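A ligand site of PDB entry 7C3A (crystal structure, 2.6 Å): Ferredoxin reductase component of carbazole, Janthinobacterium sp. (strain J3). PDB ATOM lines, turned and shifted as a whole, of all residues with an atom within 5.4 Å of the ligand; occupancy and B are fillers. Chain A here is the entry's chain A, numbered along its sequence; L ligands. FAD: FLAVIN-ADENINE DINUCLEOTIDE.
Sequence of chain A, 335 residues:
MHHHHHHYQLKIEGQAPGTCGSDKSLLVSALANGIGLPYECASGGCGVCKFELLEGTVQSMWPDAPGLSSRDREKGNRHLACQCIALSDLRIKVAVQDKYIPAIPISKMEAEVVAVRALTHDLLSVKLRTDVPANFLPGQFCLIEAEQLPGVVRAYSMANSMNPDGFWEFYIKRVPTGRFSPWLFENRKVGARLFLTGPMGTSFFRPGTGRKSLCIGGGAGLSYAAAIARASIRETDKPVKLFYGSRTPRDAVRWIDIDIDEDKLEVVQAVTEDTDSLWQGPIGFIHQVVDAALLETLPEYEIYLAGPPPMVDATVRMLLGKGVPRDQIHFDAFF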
ATOM      1  N   GLU A  40       5.869 -30.229  19.060  1.00  0.00           N
ATOM      2  CA  GLU A  40       5.493 -29.584  17.787  1.00  0.00           C
ATOM      3  C   GLU A  40       4.065 -29.039  17.851  1.00  0.00           C
ATOM      4  O   GLU A  40       3.885 -27.856  18.083  1.00  0.00           O
ATOM      5  CB  GLU A  40       5.662 -30.533  16.598  1.00  0.00           C
ATOM      6  CG  GLU A  40       7.065 -30.587  16.034  1.00  0.00           C
ATOM      7  CD  GLU A  40       7.273 -31.723  15.039  1.00  0.00           C
ATOM      8  OE1 GLU A  40       6.272 -32.202  14.443  1.00  0.00           O
ATOM      9  OE2 GLU A  40       8.437 -32.169  14.874  1.00  0.00           O
ATOM     10  N   CYS A  41       3.076 -29.896  17.648  1.00  0.00           N
ATOM     11  CA  CYS A  41       1.671 -29.477  17.642  1.00  0.00           C
ATOM     12  C   CYS A  41       1.205 -28.910  18.992  1.00  0.00           C
ATOM     13  O   CYS A  41       0.433 -27.948  19.029  1.00  0.00           O
ATOM     14  CB  CYS A  41       0.755 -30.654  17.253  1.00  0.00           C
ATOM     15  SG  CYS A  41       0.681 -32.036  18.446  1.00  0.00           S
ATOM     16  N   ALA A  42       1.693 -29.516  20.087  1.00  0.00           N
ATOM     17  CA  ALA A  42       1.198 -29.265  21.448  1.00  0.00           C
ATOM     18  C   ALA A  42      -0.283 -29.617  21.613  1.00  0.00           C
ATOM     19  O   ALA A  42      -0.938 -29.155  22.551  1.00  0.00           O
ATOM     20  CB  ALA A  42       1.476 -27.841  21.891  1.00  0.00           C
ATOM     21  N   SER A  43      -0.770 -30.467  20.707  1.00  0.00           N
ATOM     22  CA  SER A  43      -2.189 -30.805  20.629  1.00  0.00           C
ATOM     23  C   SER A  43      -2.473 -32.295  20.535  1.00  0.00           C
ATOM     24  O   SER A  43      -3.621 -32.683  20.308  1.00  0.00           O
ATOM     25  CB  SER A  43      -2.790 -30.104  19.412  1.00  0.00           C
ATOM     26  OG  SER A  43      -2.452 -28.736  19.433  1.00  0.00           O
ATOM     27  N   GLY A  44      -1.440 -33.127  20.690  1.00  0.00           N
ATOM     28  CA  GLY A  44      -1.612 -34.582  20.823  1.00  0.00           C
ATOM     29  C   GLY A  44      -1.503 -35.384  19.534  1.00  0.00           C
ATOM     30  O   GLY A  44      -1.874 -36.561  19.529  1.00  0.00           O
ATOM     31  N   MET A  61      -5.081 -35.305  29.857  1.00  0.00           N
ATOM     32  CA  MET A  61      -6.128 -34.490  29.219  1.00  0.00           C
ATOM     33  C   MET A  61      -6.916 -35.240  28.144  1.00  0.00           C
ATOM     34  O   MET A  61      -8.089 -34.945  27.907  1.00  0.00           O
ATOM     35  CB  MET A  61      -5.515 -33.243  28.572  1.00  0.00           C
ATOM     36  CG  MET A  61      -5.051 -32.171  29.543  1.00  0.00           C
ATOM     37  SD  MET A  61      -4.483 -30.641  28.677  1.00  0.00           S
ATOM     38  CE  MET A  61      -2.728 -30.953  28.588  1.00  0.00           C
ATOM     39  N   TRP A  62      -6.269 -36.208  27.488  1.00  0.00           N
ATOM     40  CA  TRP A  62      -6.885 -36.917  26.373  1.00  0.00           C
ATOM     41  C   TRP A  62      -6.193 -38.275  26.166  1.00  0.00           C
ATOM     42  O   TRP A  62      -5.139 -38.357  25.545  1.00  0.00           O
ATOM     43  CB  TRP A  62      -6.816 -36.029  25.112  1.00  0.00           C
ATOM     44  CG  TRP A  62      -7.518 -36.526  23.902  1.00  0.00           C
ATOM     45  CD1 TRP A  62      -8.703 -37.204  23.844  1.00  0.00           C
ATOM     46  CD2 TRP A  62      -7.090 -36.339  22.542  1.00  0.00           C
ATOM     47  NE1 TRP A  62      -9.025 -37.463  22.528  1.00  0.00           N
ATOM     48  CE2 TRP A  62      -8.056 -36.945  21.714  1.00  0.00           C
ATOM     49  CE3 TRP A  62      -5.983 -35.710  21.953  1.00  0.00           C
ATOM     50  CZ2 TRP A  62      -7.944 -36.959  20.335  1.00  0.00           C
ATOM     51  CZ3 TRP A  62      -5.868 -35.725  20.606  1.00  0.00           C
ATOM     52  CH2 TRP A  62      -6.836 -36.333  19.787  1.00  0.00           C
ATOM     53  N   GLN A  83      -0.113 -33.557  26.805  1.00  0.00           N
ATOM     54  CA  GLN A  83      -1.410 -34.073  27.208  1.00  0.00           C
ATOM     55  C   GLN A  83      -1.461 -34.531  28.693  1.00  0.00           C
ATOM     56  O   GLN A  83      -2.401 -35.227  29.088  1.00  0.00           O
ATOM     57  CB  GLN A  83      -1.779 -35.232  26.294  1.00  0.00           C
ATOM     58  CG  GLN A  83      -1.976 -34.865  24.834  1.00  0.00           C
ATOM     59  CD  GLN A  83      -3.062 -33.830  24.590  1.00  0.00           C
ATOM     60  OE1 GLN A  83      -2.913 -32.967  23.715  1.00  0.00           O
ATOM     61  NE2 GLN A  83      -4.161 -33.898  25.342  1.00  0.00           N
ATOM     62  N   PHE A 141       2.667 -19.556  17.780  1.00  0.00           N
ATOM     63  CA  PHE A 141       1.266 -19.702  18.174  1.00  0.00           C
ATOM     64  C   PHE A 141       1.050 -19.622  19.678  1.00  0.00           C
ATOM     65  O   PHE A 141       2.000 -19.721  20.452  1.00  0.00           O
ATOM     66  CB  PHE A 141       0.677 -21.014  17.623  1.00  0.00           C
ATOM     67  CG  PHE A 141       1.276 -22.244  18.217  1.00  0.00           C
ATOM     68  CD1 PHE A 141       2.446 -22.789  17.726  1.00  0.00           C
ATOM     69  CD2 PHE A 141       0.655 -22.863  19.305  1.00  0.00           C
ATOM     70  CE1 PHE A 141       2.997 -23.927  18.285  1.00  0.00           C
ATOM     71  CE2 PHE A 141       1.189 -23.999  19.882  1.00  0.00           C
ATOM     72  CZ  PHE A 141       2.358 -24.532  19.382  1.00  0.00           C
ATOM     73  N   GLY A 151     -11.229 -27.775  29.862  1.00  0.00           N
ATOM     74  CA  GLY A 151     -10.499 -28.912  29.297  1.00  0.00           C
ATOM     75  C   GLY A 151     -10.369 -28.853  27.790  1.00  0.00           C
ATOM     76  O   GLY A 151     -10.195 -29.893  27.147  1.00  0.00           O
ATOM     77  N   VAL A 152     -10.449 -27.644  27.229  1.00  0.00           N
ATOM     78  CA  VAL A 152     -10.278 -27.477  25.790  1.00  0.00           C
ATOM     79  C   VAL A 152      -9.328 -26.291  25.525  1.00  0.00           C
ATOM     80  O   VAL A 152      -9.715 -25.133  25.585  1.00  0.00           O
ATOM     81  CB  VAL A 152     -11.630 -27.380  25.035  1.00  0.00           C
ATOM     82  CG1 VAL A 152     -12.728 -26.809  25.909  1.00  0.00           C
ATOM     83  CG2 VAL A 152     -11.515 -26.597  23.714  1.00  0.00           C
ATOM     84  N   VAL A 153      -8.077 -26.650  25.249  1.00  0.00           N
ATOM     85  CA  VAL A 153      -7.037 -25.710  24.877  1.00  0.00           C
ATOM     86  C   VAL A 153      -6.797 -25.955  23.391  1.00  0.00           C
ATOM     87  O   VAL A 153      -6.823 -27.116  22.953  1.00  0.00           O
ATOM     88  CB  VAL A 153      -5.733 -25.921  25.716  1.00  0.00           C
ATOM     89  CG1 VAL A 153      -6.078 -26.393  27.126  1.00  0.00           C
ATOM     90  CG2 VAL A 153      -4.786 -26.931  25.075  1.00  0.00           C
ATOM     91  N   ARG A 154      -6.579 -24.897  22.596  1.00  0.00           N
ATOM     92  CA  ARG A 154      -6.438 -25.055  21.146  1.00  0.00           C
ATOM     93  C   ARG A 154      -5.385 -24.134  20.556  1.00  0.00           C
ATOM     94  O   ARG A 154      -5.439 -22.936  20.713  1.00  0.00           O
ATOM     95  CB  ARG A 154      -7.767 -24.791  20.445  1.00  0.00           C
ATOM     96  CG  ARG A 154      -8.872 -25.785  20.764  1.00  0.00           C
ATOM     97  CD  ARG A 154      -8.572 -27.189  20.280  1.00  0.00           C
ATOM     98  NE  ARG A 154      -9.777 -27.994  20.226  1.00  0.00           N
ATOM     99  CZ  ARG A 154     -10.193 -28.842  21.172  1.00  0.00           C
ATOM    100  NH1 ARG A 154      -9.485 -29.047  22.281  1.00  0.00           N
ATOM    101  NH2 ARG A 154     -11.340 -29.504  20.990  1.00  0.00           N
ATOM    102  N   ALA A 155      -4.432 -24.703  19.848  1.00  0.00           N
ATOM    103  CA  ALA A 155      -3.374 -23.925  19.191  1.00  0.00           C
ATOM    104  C   ALA A 155      -3.910 -23.062  18.037  1.00  0.00           C
ATOM    105  O   ALA A 155      -4.697 -23.533  17.218  1.00  0.00           O
ATOM    106  CB  ALA A 155      -2.258 -24.827  18.708  1.00  0.00           C
ATOM    107  N   TYR A 156      -3.494 -21.799  18.005  1.00  0.00           N
ATOM    108  CA  TYR A 156      -3.846 -20.883  16.951  1.00  0.00           C
ATOM    109  C   TYR A 156      -2.663 -20.005  16.587  1.00  0.00           C
ATOM    110  O   TYR A 156      -2.089 -19.342  17.436  1.00  0.00           O
ATOM    111  CB  TYR A 156      -5.039 -20.028  17.378  1.00  0.00           C
ATOM    112  CG  TYR A 156      -6.332 -20.791  17.427  1.00  0.00           C
ATOM    113  CD1 TYR A 156      -6.968 -21.201  16.257  1.00  0.00           C
ATOM    114  CD2 TYR A 156      -6.937 -21.101  18.635  1.00  0.00           C
ATOM    115  CE1 TYR A 156      -8.156 -21.922  16.305  1.00  0.00           C
ATOM    116  CE2 TYR A 156      -8.121 -21.811  18.696  1.00  0.00           C
ATOM    117  CZ  TYR A 156      -8.728 -22.221  17.542  1.00  0.00           C
ATOM    118  OH  TYR A 156      -9.909 -22.920  17.616  1.00  0.00           O
ATOM    119  N   SER A 157      -2.311 -19.996  15.304  1.00  0.00           N
ATOM    120  CA  SER A 157      -1.168 -19.210  14.812  1.00  0.00           C
ATOM    121  C   SER A 157      -1.448 -17.715  14.860  1.00  0.00           C
ATOM    122  O   SER A 157      -2.550 -17.274  14.529  1.00  0.00           O
ATOM    123  CB  SER A 157      -0.789 -19.642  13.396  1.00  0.00           C
ATOM    124  OG  SER A 157      -0.258 -20.962  13.359  1.00  0.00           O
ATOM    125  N   TYR A 171      -6.556 -15.856  12.948  1.00  0.00           N
ATOM    126  CA  TYR A 171      -7.632 -16.240  12.052  1.00  0.00           C
ATOM    127  C   TYR A 171      -8.054 -17.621  12.508  1.00  0.00           C
ATOM    128  O   TYR A 171      -7.217 -18.533  12.566  1.00  0.00           O
ATOM    129  CB  TYR A 171      -7.180 -16.259  10.568  1.00  0.00           C
ATOM    130  CG  TYR A 171      -6.487 -14.984  10.077  1.00  0.00           C
ATOM    131  CD1 TYR A 171      -6.902 -13.729  10.500  1.00  0.00           C
ATOM    132  CD2 TYR A 171      -5.427 -15.048   9.169  1.00  0.00           C
ATOM    133  CE1 TYR A 171      -6.263 -12.576  10.049  1.00  0.00           C
ATOM    134  CE2 TYR A 171      -4.790 -13.897   8.728  1.00  0.00           C
ATOM    135  CZ  TYR A 171      -5.207 -12.676   9.166  1.00  0.00           C
ATOM    136  OH  TYR A 171      -4.592 -11.535   8.739  1.00  0.00           O
ATOM    137  N   ILE A 172      -9.319 -17.776  12.899  1.00  0.00           N
ATOM    138  CA  ILE A 172      -9.842 -19.109  13.218  1.00  0.00           C
ATOM    139  C   ILE A 172     -10.900 -19.527  12.185  1.00  0.00           C
ATOM    140  O   ILE A 172     -11.744 -18.729  11.794  1.00  0.00           O
ATOM    141  CB  ILE A 172     -10.346 -19.240  14.696  1.00  0.00           C
ATOM    142  CG1 ILE A 172     -11.840 -18.916  14.863  1.00  0.00           C
ATOM    143  CG2 ILE A 172      -9.491 -18.409  15.655  1.00  0.00           C
ATOM    144  CD1 ILE A 172     -12.185 -17.442  14.737  1.00  0.00           C
ATOM    145  N   LYS A 173     -10.807 -20.779  11.725  1.00  0.00           N
ATOM    146  CA  LYS A 173     -11.770 -21.330  10.772  1.00  0.00           C
ATOM    147  C   LYS A 173     -12.877 -22.082  11.526  1.00  0.00           C
ATOM    148  O   LYS A 173     -12.594 -22.760  12.504  1.00  0.00           O
ATOM    149  CB  LYS A 173     -11.062 -22.287   9.799  1.00  0.00           C
ATOM    150  CG  LYS A 173     -11.892 -22.673   8.581  1.00  0.00           C
ATOM    151  CD  LYS A 173     -11.036 -23.199   7.446  1.00  0.00           C
ATOM    152  CE  LYS A 173     -11.885 -23.651   6.265  1.00  0.00           C
ATOM    153  NZ  LYS A 173     -12.572 -24.954   6.492  1.00  0.00           N
ATOM    154  N   VAL A 175     -15.275 -24.945  12.405  1.00  0.00           N
ATOM    155  CA  VAL A 175     -15.415 -26.382  12.237  1.00  0.00           C
ATOM    156  C   VAL A 175     -16.661 -26.864  12.968  1.00  0.00           C
ATOM    157  O   VAL A 175     -16.652 -27.004  14.200  1.00  0.00           O
ATOM    158  CB  VAL A 175     -14.209 -27.160  12.811  1.00  0.00           C
ATOM    159  CG1 VAL A 175     -14.119 -28.537  12.173  1.00  0.00           C
ATOM    160  CG2 VAL A 175     -12.913 -26.391  12.587  1.00  0.00           C
ATOM    161  N   THR A 177     -18.875 -29.730  14.341  1.00  0.00           N
ATOM    162  CA  THR A 177     -18.380 -30.989  14.909  1.00  0.00           C
ATOM    163  C   THR A 177     -17.233 -30.714  15.894  1.00  0.00           C
ATOM    164  O   THR A 177     -16.746 -31.637  16.550  1.00  0.00           O
ATOM    165  CB  THR A 177     -17.961 -32.043  13.837  1.00  0.00           C
ATOM    166  OG1 THR A 177     -18.440 -33.331  14.215  1.00  0.00           O
ATOM    167  CG2 THR A 177     -16.429 -32.109  13.620  1.00  0.00           C
ATOM    168  N   GLY A 178     -16.815 -29.461  15.984  1.00  0.00           N
ATOM    169  CA  GLY A 178     -15.753 -29.063  16.911  1.00  0.00           C
ATOM    170  C   GLY A 178     -16.317 -28.520  18.204  1.00  0.00           C
ATOM    171  O   GLY A 178     -17.530 -28.373  18.358  1.00  0.00           O
ATOM    172  N   ARG A 179     -15.423 -28.212  19.142  1.00  0.00           N
ATOM    173  CA  ARG A 179     -15.810 -27.674  20.440  1.00  0.00           C
ATOM    174  C   ARG A 179     -15.550 -26.191  20.507  1.00  0.00           C
ATOM    175  O   ARG A 179     -16.466 -25.414  20.761  1.00  0.00           O
ATOM    176  CB  ARG A 179     -15.040 -28.396  21.555  1.00  0.00           C
ATOM    177  CG  ARG A 179     -15.218 -29.905  21.542  1.00  0.00           C
ATOM    178  CD  ARG A 179     -14.948 -30.483  22.908  1.00  0.00           C
ATOM    179  NE  ARG A 179     -15.875 -29.917  23.890  1.00  0.00           N
ATOM    180  CZ  ARG A 179     -15.861 -30.181  25.195  1.00  0.00           C
ATOM    181  NH1 ARG A 179     -14.984 -31.044  25.716  1.00  0.00           N
ATOM    182  NH2 ARG A 179     -16.754 -29.608  25.999  1.00  0.00           N
ATOM    183  N   PHE A 180     -14.307 -25.778  20.282  1.00  0.00           N
ATOM    184  CA  PHE A 180     -13.917 -24.372  20.466  1.00  0.00           C
ATOM    185  C   PHE A 180     -14.306 -23.460  19.310  1.00  0.00           C
ATOM    186  O   PHE A 180     -14.640 -22.295  19.527  1.00  0.00           O
ATOM    187  CB  PHE A 180     -12.424 -24.256  20.698  1.00  0.00           C
ATOM    188  CG  PHE A 180     -11.988 -22.886  21.123  1.00  0.00           C
ATOM    189  CD1 PHE A 180     -12.192 -22.459  22.431  1.00  0.00           C
ATOM    190  CD2 PHE A 180     -11.396 -22.014  20.230  1.00  0.00           C
ATOM    191  CE1 PHE A 180     -11.799 -21.190  22.830  1.00  0.00           C
ATOM    192  CE2 PHE A 180     -10.991 -20.751  20.630  1.00  0.00           C
ATOM    193  CZ  PHE A 180     -11.200 -20.337  21.935  1.00  0.00           C
ATOM    194  N   SER A 181     -14.240 -23.961  18.085  1.00  0.00           N
ATOM    195  CA  SER A 181     -14.492 -23.134  16.912  1.00  0.00           C
ATOM    196  C   SER A 181     -15.935 -22.627  16.842  1.00  0.00           C
ATOM    197  O   SER A 181     -16.145 -21.453  16.557  1.00  0.00           O
ATOM    198  CB  SER A 181     -14.117 -23.884  15.625  1.00  0.00           C
ATOM    199  OG  SER A 181     -14.416 -23.091  14.509  1.00  0.00           O
ATOM    200  N   PRO A 182     -16.925 -23.505  17.111  1.00  0.00           N
ATOM    201  CA  PRO A 182     -18.298 -22.993  17.181  1.00  0.00           C
ATOM    202  C   PRO A 182     -18.540 -22.224  18.478  1.00  0.00           C
ATOM    203  O   PRO A 182     -19.358 -22.616  19.294  1.00  0.00           O
ATOM    204  CB  PRO A 182     -19.160 -24.274  17.095  1.00  0.00           C
ATOM    205  CG  PRO A 182     -18.218 -25.379  16.758  1.00  0.00           C
ATOM    206  CD  PRO A 182     -16.884 -24.964  17.278  1.00  0.00           C
ATOM    207  N   ALA A 220      -6.827 -22.832   7.061  1.00  0.00           N
ATOM    208  CA  ALA A 220      -6.609 -21.869   8.147  1.00  0.00           C
ATOM    209  C   ALA A 220      -5.137 -21.496   8.306  1.00  0.00           C
ATOM    210  O   ALA A 220      -4.813 -20.519   8.991  1.00  0.00           O
ATOM    211  CB  ALA A 220      -7.103 -22.436   9.468  1.00  0.00           C
ATOM    212  N   SER A 223      -2.814 -17.694   8.447  1.00  0.00           N
ATOM    213  CA  SER A 223      -2.200 -16.929   9.531  1.00  0.00           C
ATOM    214  C   SER A 223      -0.692 -17.102   9.548  1.00  0.00           C
ATOM    215  O   SER A 223       0.063 -16.132   9.484  1.00  0.00           O
ATOM    216  CB  SER A 223      -2.761 -17.375  10.889  1.00  0.00           C
ATOM    217  OG  SER A 223      -4.171 -17.380  10.881  1.00  0.00           O
ATOM    218  N   ASP A 332       4.265 -26.080  10.553  1.00  0.00           N
ATOM    219  CA  ASP A 332       3.394 -26.446  11.684  1.00  0.00           C
ATOM    220  C   ASP A 332       2.122 -27.106  11.154  1.00  0.00           C
ATOM    221  O   ASP A 332       1.327 -26.455  10.468  1.00  0.00           O
ATOM    222  CB  ASP A 332       2.983 -25.205  12.510  1.00  0.00           C
ATOM    223  CG  ASP A 332       3.878 -24.953  13.718  1.00  0.00           C
ATOM    224  OD1 ASP A 332       4.582 -25.877  14.150  1.00  0.00           O
ATOM    225  OD2 ASP A 332       3.855 -23.809  14.235  1.00  0.00           O
ATOM    226  N   ALA A 333       1.953 -28.390  11.443  1.00  0.00           N
ATOM    227  CA  ALA A 333       0.776 -29.139  11.011  1.00  0.00           C
ATOM    228  C   ALA A 333      -0.385 -28.949  11.992  1.00  0.00           C
ATOM    229  O   ALA A 333      -0.251 -29.221  13.196  1.00  0.00           O
ATOM    230  CB  ALA A 333       1.119 -30.611  10.866  1.00  0.00           C
ATOM    231  N   PHE A 334      -1.541 -28.524  11.480  1.00  0.00           N
ATOM    232  CA  PHE A 334      -2.681 -28.128  12.305  1.00  0.00           C
ATOM    233  C   PHE A 334      -3.450 -29.332  12.854  1.00  0.00           C
ATOM    234  O   PHE A 334      -4.619 -29.543  12.498  1.00  0.00           O
ATOM    235  CB  PHE A 334      -3.623 -27.213  11.510  1.00  0.00           C
ATOM    236  CG  PHE A 334      -3.150 -25.779  11.395  1.00  0.00           C
ATOM    237  CD1 PHE A 334      -1.840 -25.417  11.673  1.00  0.00           C
ATOM    238  CD2 PHE A 334      -4.038 -24.789  10.977  1.00  0.00           C
ATOM    239  CE1 PHE A 334      -1.425 -24.092  11.557  1.00  0.00           C
ATOM    240  CE2 PHE A 334      -3.637 -23.481  10.856  1.00  0.00           C
ATOM    241  CZ  PHE A 334      -2.329 -23.121  11.143  1.00  0.00           C
ATOM    242  N   PHE A 335      -2.808 -30.093  13.727  1.00  0.00           N
ATOM    243  CA  PHE A 335      -3.461 -31.200  14.442  1.00  0.00           C
ATOM    244  C   PHE A 335      -4.545 -30.626  15.341  1.00  0.00           C
ATOM    245  O   PHE A 335      -4.307 -30.333  16.511  1.00  0.00           O
ATOM    246  CB  PHE A 335      -2.454 -31.996  15.282  1.00  0.00           C
ATOM    247  CG  PHE A 335      -1.591 -32.939  14.490  1.00  0.00           C
ATOM    248  CD1 PHE A 335      -2.101 -34.129  14.007  1.00  0.00           C
ATOM    249  CD2 PHE A 335      -0.247 -32.648  14.265  1.00  0.00           C
ATOM    250  CE1 PHE A 335      -1.294 -35.005  13.287  1.00  0.00           C
ATOM    251  CE2 PHE A 335       0.560 -33.524  13.545  1.00  0.00           C
ATOM    252  CZ  PHE A 335       0.028 -34.711  13.058  1.00  0.00           C
ATOM    253  OXT PHE A 335      -5.695 -30.414  14.938  1.00  0.00           O
HETATM  254  PA  FAD L   1     -12.506 -30.096  17.560  1.00  0.00           P
HETATM  255  O1A FAD L   1     -12.940 -31.115  16.491  1.00  0.00           O
HETATM  256  O2A FAD L   1     -13.279 -29.896  18.842  1.00  0.00           O
HETATM  257  O5B FAD L   1     -10.988 -30.396  17.952  1.00  0.00           O
HETATM  258  C5B FAD L   1     -10.106 -30.835  16.920  1.00  0.00           C
HETATM  259  C4B FAD L   1      -8.675 -30.878  17.433  1.00  0.00           C
HETATM  260  O4B FAD L   1      -8.602 -30.673  18.842  1.00  0.00           O
HETATM  261  C3B FAD L   1      -8.008 -32.216  17.131  1.00  0.00           C
HETATM  262  O3B FAD L   1      -7.329 -32.206  15.865  1.00  0.00           O
HETATM  263  C2B FAD L   1      -7.069 -32.397  18.293  1.00  0.00           C
HETATM  264  O2B FAD L   1      -5.806 -31.766  18.017  1.00  0.00           O
HETATM  265  C1B FAD L   1      -7.753 -31.662  19.439  1.00  0.00           C
HETATM  266  N9A FAD L   1      -8.561 -32.581  20.258  1.00  0.00           N
HETATM  267  C8A FAD L   1      -9.340 -33.624  19.828  1.00  0.00           C
HETATM  268  N7A FAD L   1      -9.942 -34.233  20.879  1.00  0.00           N
HETATM  269  C5A FAD L   1      -9.561 -33.586  22.007  1.00  0.00           C
HETATM  270  C6A FAD L   1      -9.836 -33.720  23.460  1.00  0.00           C
HETATM  271  N6A FAD L   1     -10.653 -34.697  23.914  1.00  0.00           N
HETATM  272  N1A FAD L   1      -9.235 -32.830  24.303  1.00  0.00           N
HETATM  273  C2A FAD L   1      -8.409 -31.850  23.851  1.00  0.00           C
HETATM  274  N3A FAD L   1      -8.119 -31.678  22.532  1.00  0.00           N
HETATM  275  C4A FAD L   1      -8.652 -32.500  21.591  1.00  0.00           C
HETATM  276  N1  FAD L   1      -6.722 -23.407  13.515  1.00  0.00           N
HETATM  277  C2  FAD L   1      -7.085 -22.199  13.018  1.00  0.00           C
HETATM  278  O2  FAD L   1      -8.278 -22.044  12.690  1.00  0.00           O
HETATM  279  N3  FAD L   1      -6.197 -21.189  12.864  1.00  0.00           N
HETATM  280  C4  FAD L   1      -4.902 -21.325  13.197  1.00  0.00           C
HETATM  281  O4  FAD L   1      -4.121 -20.358  13.044  1.00  0.00           O
HETATM  282  C4X FAD L   1      -4.446 -22.632  13.769  1.00  0.00           C
HETATM  283  N5  FAD L   1      -3.163 -22.885  14.150  1.00  0.00           N
HETATM  284  C5X FAD L   1      -2.779 -24.096  14.652  1.00  0.00           C
HETATM  285  C6  FAD L   1      -1.457 -24.300  15.019  1.00  0.00           C
HETATM  286  C7  FAD L   1      -1.048 -25.523  15.533  1.00  0.00           C
HETATM  287  C7M FAD L   1       0.394 -25.734  15.915  1.00  0.00           C
HETATM  288  C8  FAD L   1      -2.037 -26.618  15.692  1.00  0.00           C
HETATM  289  C8M FAD L   1      -1.650 -27.961  16.243  1.00  0.00           C
HETATM  290  C9  FAD L   1      -3.358 -26.425  15.334  1.00  0.00           C
HETATM  291  C9A FAD L   1      -3.764 -25.200  14.810  1.00  0.00           C
HETATM  292  N10 FAD L   1      -5.106 -24.959  14.424  1.00  0.00           N
HETATM  293  C10 FAD L   1      -5.461 -23.691  13.897  1.00  0.00           C
HETATM  294  C1' FAD L   1      -6.150 -25.975  14.554  1.00  0.00           C
HETATM  295  C2' FAD L   1      -7.118 -25.547  15.669  1.00  0.00           C
HETATM  296  O2' FAD L   1      -6.837 -26.309  16.849  1.00  0.00           O
HETATM  297  C3' FAD L   1      -8.566 -25.698  15.202  1.00  0.00           C
HETATM  298  O3' FAD L   1      -9.428 -24.713  15.774  1.00  0.00           O
HETATM  299  C4' FAD L   1      -9.126 -27.094  15.461  1.00  0.00           C
HETATM  300  O4' FAD L   1     -10.092 -27.359  14.444  1.00  0.00           O
HETATM  301  C5' FAD L   1      -9.814 -27.148  16.820  1.00  0.00           C
HETATM  302  O5' FAD L   1     -11.121 -26.574  16.728  1.00  0.00           O
HETATM  303  P   FAD L   1     -12.303 -27.245  17.564  1.00  0.00           P
HETATM  304  O1P FAD L   1     -11.826 -27.441  18.978  1.00  0.00           O
HETATM  305  O2P FAD L   1     -13.557 -26.441  17.327  1.00  0.00           O
HETATM  306  O3P FAD L   1     -12.448 -28.673  16.806  1.00  0.00           O
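NE1 of Trp 62 lies close to N6A of the ligand (3.5 Å).
O of Ala 155 sits close to N10 of the ligand.
O of Cys 41 touches C8M of the ligand (3.5 Å).
CE1 of Phe 141 touches C7M of the ligand, 3.96 Å away.
CA of Ile 172 touches O2 of the ligand (3.4 Å).
Val 175 touches the ligand (CG2 to O4', 3.5 Å).
O of Thr 177 touches O1A of the ligand, at 3.8 Å.
Gly 178 touches the ligand (CA to O2A, 3.2 Å).
Pro 182 touches the ligand.
Ala 220 touches the ligand.
OG of Ser 223 touches O4 of the ligand, at 3.7 Å.
O of Ala 333 touches C8M of the ligand (3.6 Å).
Phe 334 touches the ligand.
Hydrophobic or aromatic side chains within 4 Å of the ligand: Trp 62, Phe 141, Ala 155, Tyr 156, Val 175, Phe 180, Pro 182, Ala 220 and Phe 334.
23 residues have an atom within 4 Å of the ligand: Cys 41, Ser 43, Trp 62, Phe 141, Arg 154, Ala 155, Tyr 156, Ser 157, Tyr 171, Ile 172, Lys 173, Val 175, Thr 177, Gly 178, Arg 179, Phe 180, Ser 181, Pro 182, Ala 220, Ser 223, Ala 333, Phe 334 and Phe 335.
The nearest printed residue that does not touch the ligand is Asp 332 (4.2 Å).
N of Lys 173 is in hydrogen-bond range of O2 of the ligand.
The backbone carbonyl oxygen (O) of Ser 43 sits at hydrogen-bond distance from an oxygen (O2B) of the ligand, 3.3 Å away.
The backbone carbonyl oxygen of Tyr 171 is in hydrogen-bond range of a nitrogen (N3) of the ligand (2.9 Å).
The guanidinium group (NE) of Arg 154 lies within salt-bridge range of an oxygen (O1P) of the ligand (2.5 Å).
N of Ser 157 sits at hydrogen-bond distance from O4 of the ligand (2.9 Å).
O2P of the ligand lies within hydrogen-bond range of N of Phe 180.
The backbone NH of Arg 179 is in hydrogen-bond range of an oxygen (O2A) of the ligand, at 2.7 Å.
O2B of the ligand is in hydrogen-bond range of O of Phe 335, 2.6 Å away.
An oxygen (O3') of the ligand sits at hydrogen-bond distance from the side-chain hydroxyl (OH) of Tyr 156 (2.6 Å).
O2P of the ligand is in hydrogen-bond range of N of Ser 181 (2.7 Å).
The side-chain hydroxyl (OG) of Ser 181 is in hydrogen-bond range of the backbone NH (N) of Val 175 (2.9 Å).
The side-chain hydroxyl of Ser 43 is in hydrogen-bond range of the backbone carbonyl oxygen of Cys 41 (3.0 Å).
The backbone NH (N) of Gly 44 lies close to the side-chain sulfur (SG) of Cys 41 (3.3 Å).
The side-chain hydroxyl (OG) of Ser 181 is in hydrogen-bond range of the backbone carbonyl oxygen (O) of Lys 173 (2.7 Å).
The side-chain amide oxygen (OE1) of Gln 83 sits close to the backbone carbonyl oxygen (O) of Ser 43 (3.5 Å).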
